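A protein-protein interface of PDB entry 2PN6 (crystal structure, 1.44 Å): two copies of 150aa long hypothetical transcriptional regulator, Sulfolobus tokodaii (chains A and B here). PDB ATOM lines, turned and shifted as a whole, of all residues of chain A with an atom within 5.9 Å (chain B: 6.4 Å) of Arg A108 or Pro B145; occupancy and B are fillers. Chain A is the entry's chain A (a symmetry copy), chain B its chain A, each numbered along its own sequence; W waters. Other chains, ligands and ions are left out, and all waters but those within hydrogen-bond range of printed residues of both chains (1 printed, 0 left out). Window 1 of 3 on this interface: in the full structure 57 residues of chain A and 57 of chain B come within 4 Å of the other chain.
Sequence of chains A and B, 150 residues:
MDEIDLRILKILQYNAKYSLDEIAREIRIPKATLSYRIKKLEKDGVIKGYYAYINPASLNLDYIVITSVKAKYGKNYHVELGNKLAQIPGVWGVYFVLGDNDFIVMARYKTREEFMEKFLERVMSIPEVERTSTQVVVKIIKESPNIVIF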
ATOM      1  N   PRO A  56       4.868   9.821  -1.842  1.00  0.00           N
ATOM      2  CA  PRO A  56       6.099  10.263  -1.181  1.00  0.00           C
ATOM      3  C   PRO A  56       7.262  10.449  -2.149  1.00  0.00           C
ATOM      4  O   PRO A  56       8.113  11.309  -1.945  1.00  0.00           O
ATOM      5  CB  PRO A  56       6.357   9.154  -0.165  1.00  0.00           C
ATOM      6  CG  PRO A  56       4.972   8.723   0.197  1.00  0.00           C
ATOM      7  CD  PRO A  56       4.313   8.639  -1.161  1.00  0.00           C
ATOM      8  N   LEU A  61      11.020  11.679  -1.067  1.00  0.00           N
ATOM      9  CA  LEU A  61      11.187  10.943   0.187  1.00  0.00           C
ATOM     10  C   LEU A  61      11.675   9.547  -0.176  1.00  0.00           C
ATOM     11  O   LEU A  61      10.900   8.589  -0.229  1.00  0.00           O
ATOM     12  CB  LEU A  61       9.856  10.881   0.939  1.00  0.00           C
ATOM     13  CG  LEU A  61       9.380  12.241   1.457  1.00  0.00           C
ATOM     14  CD1 LEU A  61       7.923  12.158   1.889  1.00  0.00           C
ATOM     15  CD2 LEU A  61      10.269  12.683   2.609  1.00  0.00           C
ATOM     16  N   TYR A  63      14.520   8.124   1.415  1.00  0.00           N
ATOM     17  CA  TYR A  63      15.203   7.492   2.538  1.00  0.00           C
ATOM     18  C   TYR A  63      14.141   7.043   3.529  1.00  0.00           C
ATOM     19  O   TYR A  63      13.717   7.799   4.408  1.00  0.00           O
ATOM     20  CB  TYR A  63      16.184   8.462   3.194  1.00  0.00           C
ATOM     21  CG  TYR A  63      17.469   7.778   3.588  1.00  0.00           C
ATOM     22  CD1 TYR A  63      18.474   7.553   2.647  1.00  0.00           C
ATOM     23  CD2 TYR A  63      17.659   7.301   4.882  1.00  0.00           C
ATOM     24  CE1 TYR A  63      19.634   6.868   2.985  1.00  0.00           C
ATOM     25  CE2 TYR A  63      18.816   6.612   5.230  1.00  0.00           C
ATOM     26  CZ  TYR A  63      19.796   6.401   4.276  1.00  0.00           C
ATOM     27  OH  TYR A  63      20.940   5.721   4.617  1.00  0.00           O
ATOM     28  N   ILE A  64      13.724   5.794   3.365  1.00  0.00           N
ATOM     29  CA  ILE A  64      12.667   5.191   4.159  1.00  0.00           C
ATOM     30  C   ILE A  64      13.244   4.219   5.176  1.00  0.00           C
ATOM     31  O   ILE A  64      13.996   3.309   4.821  1.00  0.00           O
ATOM     32  CB  ILE A  64      11.701   4.459   3.222  1.00  0.00           C
ATOM     33  CG1 ILE A  64      11.232   5.424   2.125  1.00  0.00           C
ATOM     34  CG2 ILE A  64      10.526   3.896   3.999  1.00  0.00           C
ATOM     35  CD1 ILE A  64      10.535   6.666   2.642  1.00  0.00           C
ATOM     36  N   VAL A  65      12.872   4.398   6.439  1.00  0.00           N
ATOM     37  CA  VAL A  65      13.423   3.565   7.496  1.00  0.00           C
ATOM     38  C   VAL A  65      12.402   2.994   8.468  1.00  0.00           C
ATOM     39  O   VAL A  65      11.321   3.545   8.660  1.00  0.00           O
ATOM     40  CB  VAL A  65      14.471   4.363   8.320  1.00  0.00           C
ATOM     41  CG1 VAL A  65      15.597   4.845   7.415  1.00  0.00           C
ATOM     42  CG2 VAL A  65      13.806   5.553   9.002  1.00  0.00           C
ATOM     43  N   PRO A  89      10.201  15.134  13.583  1.00  0.00           N
ATOM     44  CA  PRO A  89       9.736  15.384  12.215  1.00  0.00           C
ATOM     45  C   PRO A  89      10.149  14.220  11.316  1.00  0.00           C
ATOM     46  O   PRO A  89      11.285  13.749  11.389  1.00  0.00           O
ATOM     47  CB  PRO A  89      10.450  16.680  11.839  1.00  0.00           C
ATOM     48  CG  PRO A  89      10.599  17.376  13.155  1.00  0.00           C
ATOM     49  CD  PRO A  89      11.018  16.256  14.076  1.00  0.00           C
ATOM     50  N   GLY A  90       9.227  13.755  10.482  1.00  0.00           N
ATOM     51  CA  GLY A  90       9.532  12.649   9.590  1.00  0.00           C
ATOM     52  C   GLY A  90       9.036  11.309  10.102  1.00  0.00           C
ATOM     53  O   GLY A  90       8.905  10.361   9.332  1.00  0.00           O
ATOM     54  N   VAL A  91       8.772  11.227  11.403  1.00  0.00           N
ATOM     55  CA  VAL A  91       8.272   9.994  12.009  1.00  0.00           C
ATOM     56  C   VAL A  91       6.750   9.957  11.899  1.00  0.00           C
ATOM     57  O   VAL A  91       6.073  10.846  12.415  1.00  0.00           O
ATOM     58  CB  VAL A  91       8.669   9.911  13.504  1.00  0.00           C
ATOM     59  CG1 VAL A  91       7.897   8.786  14.198  1.00  0.00           C
ATOM     60  CG2 VAL A  91      10.163   9.677  13.627  1.00  0.00           C
ATOM     61  N   TRP A  92       6.213   8.941  11.222  1.00  0.00           N
ATOM     62  CA  TRP A  92       4.764   8.821  11.074  1.00  0.00           C
ATOM     63  C   TRP A  92       4.159   7.662  11.853  1.00  0.00           C
ATOM     64  O   TRP A  92       2.949   7.620  12.077  1.00  0.00           O
ATOM     65  CB  TRP A  92       4.351   8.705   9.596  1.00  0.00           C
ATOM     66  CG  TRP A  92       4.872   7.516   8.818  1.00  0.00           C
ATOM     67  CD1 TRP A  92       5.908   7.516   7.929  1.00  0.00           C
ATOM     68  CD2 TRP A  92       4.312   6.192   8.776  1.00  0.00           C
ATOM     69  NE1 TRP A  92       6.023   6.286   7.326  1.00  0.00           N
ATOM     70  CE2 TRP A  92       5.058   5.453   7.829  1.00  0.00           C
ATOM     71  CE3 TRP A  92       3.253   5.562   9.442  1.00  0.00           C
ATOM     72  CZ2 TRP A  92       4.779   4.114   7.528  1.00  0.00           C
ATOM     73  CZ3 TRP A  92       2.975   4.224   9.144  1.00  0.00           C
ATOM     74  CH2 TRP A  92       3.737   3.519   8.193  1.00  0.00           C
ATOM     75  N   MET A 106       8.449   4.192  12.255  1.00  0.00           N
ATOM     76  CA  MET A 106       8.415   4.310  10.802  1.00  0.00           C
ATOM     77  C   MET A 106       8.679   5.773  10.466  1.00  0.00           C
ATOM     78  O   MET A 106       8.000   6.662  10.988  1.00  0.00           O
ATOM     79  CB  MET A 106       7.035   3.933  10.260  1.00  0.00           C
ATOM     80  CG  MET A 106       6.461   2.620  10.771  1.00  0.00           C
ATOM     81  SD  MET A 106       7.338   1.158  10.189  1.00  0.00           S
ATOM     82  CE  MET A 106       6.604   0.928   8.602  1.00  0.00           C
ATOM     83  N   ALA A 107       9.656   6.027   9.600  1.00  0.00           N
ATOM     84  CA  ALA A 107       9.970   7.400   9.225  1.00  0.00           C
ATOM     85  C   ALA A 107      10.367   7.526   7.759  1.00  0.00           C
ATOM     86  O   ALA A 107      10.683   6.532   7.099  1.00  0.00           O
ATOM     87  CB  ALA A 107      11.077   7.942  10.123  1.00  0.00           C
ATOM     88  N   ARG A 108      10.334   8.760   7.259  1.00  0.00           N
ATOM     89  CA  ARG A 108      10.673   9.059   5.871  1.00  0.00           C
ATOM     90  C   ARG A 108      11.485  10.349   5.792  1.00  0.00           C
ATOM     91  O   ARG A 108      11.164  11.322   6.468  1.00  0.00           O
ATOM     92  CB  ARG A 108       9.409   9.290   5.032  1.00  0.00           C
ATOM     93  CG  ARG A 108       8.319   8.238   5.100  1.00  0.00           C
ATOM     94  CD  ARG A 108       7.299   8.526   4.003  1.00  0.00           C
ATOM     95  NE  ARG A 108       6.112   7.674   4.047  1.00  0.00           N
ATOM     96  CZ  ARG A 108       4.928   8.060   4.515  1.00  0.00           C
ATOM     97  NH1 ARG A 108       4.761   9.290   4.989  1.00  0.00           N
ATOM     98  NH2 ARG A 108       3.904   7.216   4.499  1.00  0.00           N
ATOM     99  N   TYR A 109      12.522  10.355   4.960  1.00  0.00           N
ATOM    100  CA  TYR A 109      13.350  11.546   4.752  1.00  0.00           C
ATOM    101  C   TYR A 109      13.780  11.594   3.297  1.00  0.00           C
ATOM    102  O   TYR A 109      13.637  10.614   2.569  1.00  0.00           O
ATOM    103  CB  TYR A 109      14.577  11.533   5.671  1.00  0.00           C
ATOM    104  CG  TYR A 109      14.183  11.544   7.125  1.00  0.00           C
ATOM    105  CD1 TYR A 109      13.716  12.712   7.728  1.00  0.00           C
ATOM    106  CD2 TYR A 109      14.146  10.359   7.861  1.00  0.00           C
ATOM    107  CE1 TYR A 109      13.208  12.698   9.020  1.00  0.00           C
ATOM    108  CE2 TYR A 109      13.642  10.334   9.155  1.00  0.00           C
ATOM    109  CZ  TYR A 109      13.169  11.503   9.726  1.00  0.00           C
ATOM    110  OH  TYR A 109      12.614  11.469  10.984  1.00  0.00           O
ATOM    111  N   LYS A 110      14.299  12.738   2.866  1.00  0.00           N
ATOM    112  CA  LYS A 110      14.730  12.872   1.483  1.00  0.00           C
ATOM    113  C   LYS A 110      16.113  12.290   1.251  1.00  0.00           C
ATOM    114  O   LYS A 110      16.372  11.694   0.205  1.00  0.00           O
ATOM    115  CB  LYS A 110      14.713  14.345   1.062  1.00  0.00           C
ATOM    116  CG  LYS A 110      13.315  14.923   0.941  1.00  0.00           C
ATOM    117  CD  LYS A 110      13.345  16.413   0.636  1.00  0.00           C
ATOM    118  CE  LYS A 110      11.944  16.950   0.394  1.00  0.00           C
ATOM    119  NZ  LYS A 110      11.910  18.436   0.302  1.00  0.00           N
ATOM    120  N   GLU A 114      19.686  14.207   5.851  1.00  0.00           N
ATOM    121  CA  GLU A 114      18.491  14.706   6.526  1.00  0.00           C
ATOM    122  C   GLU A 114      18.095  13.715   7.618  1.00  0.00           C
ATOM    123  O   GLU A 114      17.723  14.095   8.726  1.00  0.00           O
ATOM    124  CB  GLU A 114      17.343  14.853   5.526  1.00  0.00           C
ATOM    125  CG  GLU A 114      16.095  15.486   6.111  1.00  0.00           C
ATOM    126  CD  GLU A 114      14.921  15.453   5.152  1.00  0.00           C
ATOM    127  OE1 GLU A 114      15.132  15.151   3.959  1.00  0.00           O
ATOM    128  OE2 GLU A 114      13.788  15.736   5.588  1.00  0.00           O
ATOM    129  N   GLU A 143       2.157  -0.346   0.607  1.00  0.00           N
ATOM    130  CA  GLU A 143       1.950   0.562   1.725  1.00  0.00           C
ATOM    131  C   GLU A 143       0.584   1.193   1.525  1.00  0.00           C
ATOM    132  O   GLU A 143       0.459   2.286   0.974  1.00  0.00           O
ATOM    133  CB  GLU A 143       3.034   1.642   1.814  1.00  0.00           C
ATOM    134  CG  GLU A 143       2.854   2.528   3.051  1.00  0.00           C
ATOM    135  CD  GLU A 143       3.986   3.510   3.271  1.00  0.00           C
ATOM    136  OE1 GLU A 143       5.020   3.125   3.857  1.00  0.00           O
ATOM    137  OE2 GLU A 143       3.842   4.679   2.856  1.00  0.00           O
ATOM    138  N   PRO A 145      -2.069   1.588   4.184  1.00  0.00           N
ATOM    139  CA  PRO A 145      -2.683   1.569   5.516  1.00  0.00           C
ATOM    140  C   PRO A 145      -4.138   2.029   5.523  1.00  0.00           C
ATOM    141  O   PRO A 145      -4.861   1.815   6.496  1.00  0.00           O
ATOM    142  CB  PRO A 145      -1.773   2.486   6.329  1.00  0.00           C
ATOM    143  CG  PRO A 145      -1.281   3.466   5.310  1.00  0.00           C
ATOM    144  CD  PRO A 145      -0.980   2.578   4.121  1.00  0.00           C
ATOM    145  N   TRP B  92      -1.224  -4.709   5.103  1.00  0.00           N
ATOM    146  CA  TRP B  92      -1.257  -3.412   4.429  1.00  0.00           C
ATOM    147  C   TRP B  92       0.118  -2.865   4.077  1.00  0.00           C
ATOM    148  O   TRP B  92       0.241  -1.960   3.250  1.00  0.00           O
ATOM    149  CB  TRP B  92      -2.023  -2.362   5.254  1.00  0.00           C
ATOM    150  CG  TRP B  92      -1.476  -2.019   6.623  1.00  0.00           C
ATOM    151  CD1 TRP B  92      -1.952  -2.465   7.824  1.00  0.00           C
ATOM    152  CD2 TRP B  92      -0.435  -1.078   6.932  1.00  0.00           C
ATOM    153  NE1 TRP B  92      -1.286  -1.854   8.859  1.00  0.00           N
ATOM    154  CE2 TRP B  92      -0.346  -1.000   8.342  1.00  0.00           C
ATOM    155  CE3 TRP B  92       0.429  -0.293   6.158  1.00  0.00           C
ATOM    156  CZ2 TRP B  92       0.569  -0.167   8.996  1.00  0.00           C
ATOM    157  CZ3 TRP B  92       1.345   0.539   6.810  1.00  0.00           C
ATOM    158  CH2 TRP B  92       1.403   0.593   8.215  1.00  0.00           C
ATOM    159  N   GLU B 143       0.175   6.686  14.245  1.00  0.00           N
ATOM    160  CA  GLU B 143       0.064   6.030  12.951  1.00  0.00           C
ATOM    161  C   GLU B 143      -0.611   7.019  12.019  1.00  0.00           C
ATOM    162  O   GLU B 143      -1.826   6.989  11.827  1.00  0.00           O
ATOM    163  CB  GLU B 143      -0.734   4.723  13.020  1.00  0.00           C
ATOM    164  CG  GLU B 143      -0.757   3.998  11.670  1.00  0.00           C
ATOM    165  CD  GLU B 143      -1.399   2.628  11.722  1.00  0.00           C
ATOM    166  OE1 GLU B 143      -0.714   1.649  12.089  1.00  0.00           O
ATOM    167  OE2 GLU B 143      -2.599   2.525  11.391  1.00  0.00           O
ATOM    168  N   SER B 144       0.202   7.907  11.460  1.00  0.00           N
ATOM    169  CA  SER B 144      -0.278   8.946  10.556  1.00  0.00           C
ATOM    170  C   SER B 144       0.548   8.952   9.271  1.00  0.00           C
ATOM    171  O   SER B 144       1.218   9.939   8.955  1.00  0.00           O
ATOM    172  CB  SER B 144      -0.179  10.311  11.241  1.00  0.00           C
ATOM    173  OG  SER B 144      -0.966  10.355  12.421  1.00  0.00           O
ATOM    174  N   PRO B 145       0.501   7.847   8.506  1.00  0.00           N
ATOM    175  CA  PRO B 145       1.260   7.751   7.253  1.00  0.00           C
ATOM    176  C   PRO B 145       0.839   8.779   6.207  1.00  0.00           C
ATOM    177  O   PRO B 145       1.548   9.004   5.226  1.00  0.00           O
ATOM    178  CB  PRO B 145       1.003   6.316   6.803  1.00  0.00           C
ATOM    179  CG  PRO B 145      -0.368   6.032   7.335  1.00  0.00           C
ATOM    180  CD  PRO B 145      -0.311   6.636   8.722  1.00  0.00           C
ATOM    181  N   ASN B 146      -0.312   9.404   6.426  1.00  0.00           N
ATOM    182  CA  ASN B 146      -0.819  10.413   5.502  1.00  0.00           C
ATOM    183  C   ASN B 146       0.005  11.698   5.538  1.00  0.00           C
ATOM    184  O   ASN B 146       0.000  12.466   4.576  1.00  0.00           O
ATOM    185  CB  ASN B 146      -2.275  10.738   5.836  1.00  0.00           C
ATOM    186  CG  ASN B 146      -2.458  11.146   7.283  1.00  0.00           C
ATOM    187  OD1 ASN B 146      -2.198  10.360   8.196  1.00  0.00           O
ATOM    188  ND2 ASN B 146      -2.901  12.379   7.504  1.00  0.00           N
ATOM    189  N   ILE B 147       0.699  11.940   6.647  1.00  0.00           N
ATOM    190  CA  ILE B 147       1.517  13.142   6.784  1.00  0.00           C
ATOM    191  C   ILE B 147       2.859  12.950   6.086  1.00  0.00           C
ATOM    192  O   ILE B 147       3.746  12.263   6.596  1.00  0.00           O
ATOM    193  CB  ILE B 147       1.768  13.493   8.270  1.00  0.00           C
ATOM    194  CG1 ILE B 147       0.432  13.693   8.993  1.00  0.00           C
ATOM    195  CG2 ILE B 147       2.613  14.762   8.376  1.00  0.00           C
ATOM    196  CD1 ILE B 147      -0.454  14.770   8.379  1.00  0.00           C
ATOM    197  N   VAL B 148       3.003  13.555   4.913  1.00  0.00           N
ATOM    198  CA  VAL B 148       4.239  13.446   4.143  1.00  0.00           C
ATOM    199  C   VAL B 148       5.082  14.716   4.205  1.00  0.00           C
ATOM    200  O   VAL B 148       6.274  14.688   3.928  1.00  0.00           O
ATOM    201  CB  VAL B 148       3.945  13.107   2.670  1.00  0.00           C
ATOM    202  CG1 VAL B 148       3.443  11.671   2.552  1.00  0.00           C
ATOM    203  CG2 VAL B 148       2.913  14.070   2.120  1.00  0.00           C
ATOM    204  N   PHE B 150       6.136  17.669   6.859  1.00  0.00           N
ATOM    205  CA  PHE B 150       6.100  18.115   8.256  1.00  0.00           C
ATOM    206  C   PHE B 150       6.280  19.630   8.392  1.00  0.00           C
ATOM    207  O   PHE B 150       7.246  20.050   9.059  1.00  0.00           O
ATOM    208  CB  PHE B 150       7.174  17.391   9.065  1.00  0.00           C
ATOM    209  CG  PHE B 150       6.867  15.947   9.301  1.00  0.00           C
ATOM    210  CD1 PHE B 150       6.855  15.044   8.245  1.00  0.00           C
ATOM    211  CD2 PHE B 150       6.508  15.506  10.566  1.00  0.00           C
ATOM    212  CE1 PHE B 150       6.479  13.719   8.448  1.00  0.00           C
ATOM    213  CE2 PHE B 150       6.134  14.198  10.777  1.00  0.00           C
ATOM    214  CZ  PHE B 150       6.114  13.301   9.725  1.00  0.00           C
ATOM    215  OXT PHE B 150       5.444  20.372   7.838  1.00  0.00           O
HETATM  216  O   HOH W   1       3.180  11.614  10.746  1.00  0.00           O
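The backbone carbonyl oxygen of Pro B145 is in hydrogen-bond range of the guanidinium group of Arg A108, 3.0 Å away. N of Ser B144 lies within hydrogen-bond range of O of Trp A92, 2.8 Å away.
NH2 of Arg A108 is in salt-bridge range of OE2 of Glu A143 (3.0 Å). O of Pro A56 sits at hydrogen-bond distance from N of Leu A61 (3.1 Å). O of Pro A89 lies within hydrogen-bond range of OH of Tyr A109. The backbone NH (N) of Trp A92 lies within hydrogen-bond range of the backbone carbonyl oxygen (O) of Met A106, at 2.9 Å. O of Gly A90 is in hydrogen-bond range of N of Arg A108.
Among the printed residues, merely in contact across the chains: Leu A61 with Val B148, Pro A89 with Phe B150, Gly A90 with Phe B150, Val A91 with Phe B150, Trp A92 with Trp B92, Trp A92 with Glu B143, Trp A92 with Pro B145, Arg A108 with Ile B147, Arg A108 with Val B148, Glu A143 with Trp B92, Pro A145 with Trp B92 and Pro A145 with Pro B145.
Tyr A63 touches none of the printed residues of chain B. Of the printed residues of chain B, Pro A89 touches Phe B150. Printed residues of chain B within 4 Å of Arg A108: Pro B145 (3.0 Å), Ile B147 (3.5 Å) and Val B148 (3.7 Å). Of the printed residues of chain A, Trp B92 touches Trp A92, Glu A143 and Pro A145. Of chain A, only Trp A92 (3.5 Å), Arg A108 (3.0 Å) and Pro A145 (3.4 Å) come within 4 Å of Pro B145. Printed residues of chain A within 4 Å of Phe B150: Pro A89 (3.6 Å), Gly A90 (3.1 Å) and Val A91 (3.6 Å). The nearest printed residue of chain B that does not touch Arg A108 is Asn B146 (5.1 Å). The nearest printed residue of chain A that does not touch Val B148 is Pro A56 (4.1 Å).
Of the 8 printed residues of chain B, 7 touch a printed residue of chain A. Printed residues of chain A that touch a printed residue of chain B: Leu A61, Pro A89, Gly A90, Val A91, Trp A92, Arg A108, Glu A143 and Pro A145.
Trp B92 touches its own counterpart, Trp A92. Trp A92 touches Glu B143, and with the chains exchanged Glu A143 touches Trp B92. Trp A92 touches Pro B145, and with the chains exchanged Pro A145 touches Trp B92. Pro A145 touches its own counterpart, Pro B145. 3 positions are printed for both chains. Of the 14 pairs that touch across the chains among the printed residues, 6 have their exchanged pair printed and touching as well.
Water W1 bridges the backbone carbonyl oxygen (O) of Ser B144 (3.1 Å) and the backbone carbonyl oxygen (O) of Val A91 (3.4 Å).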
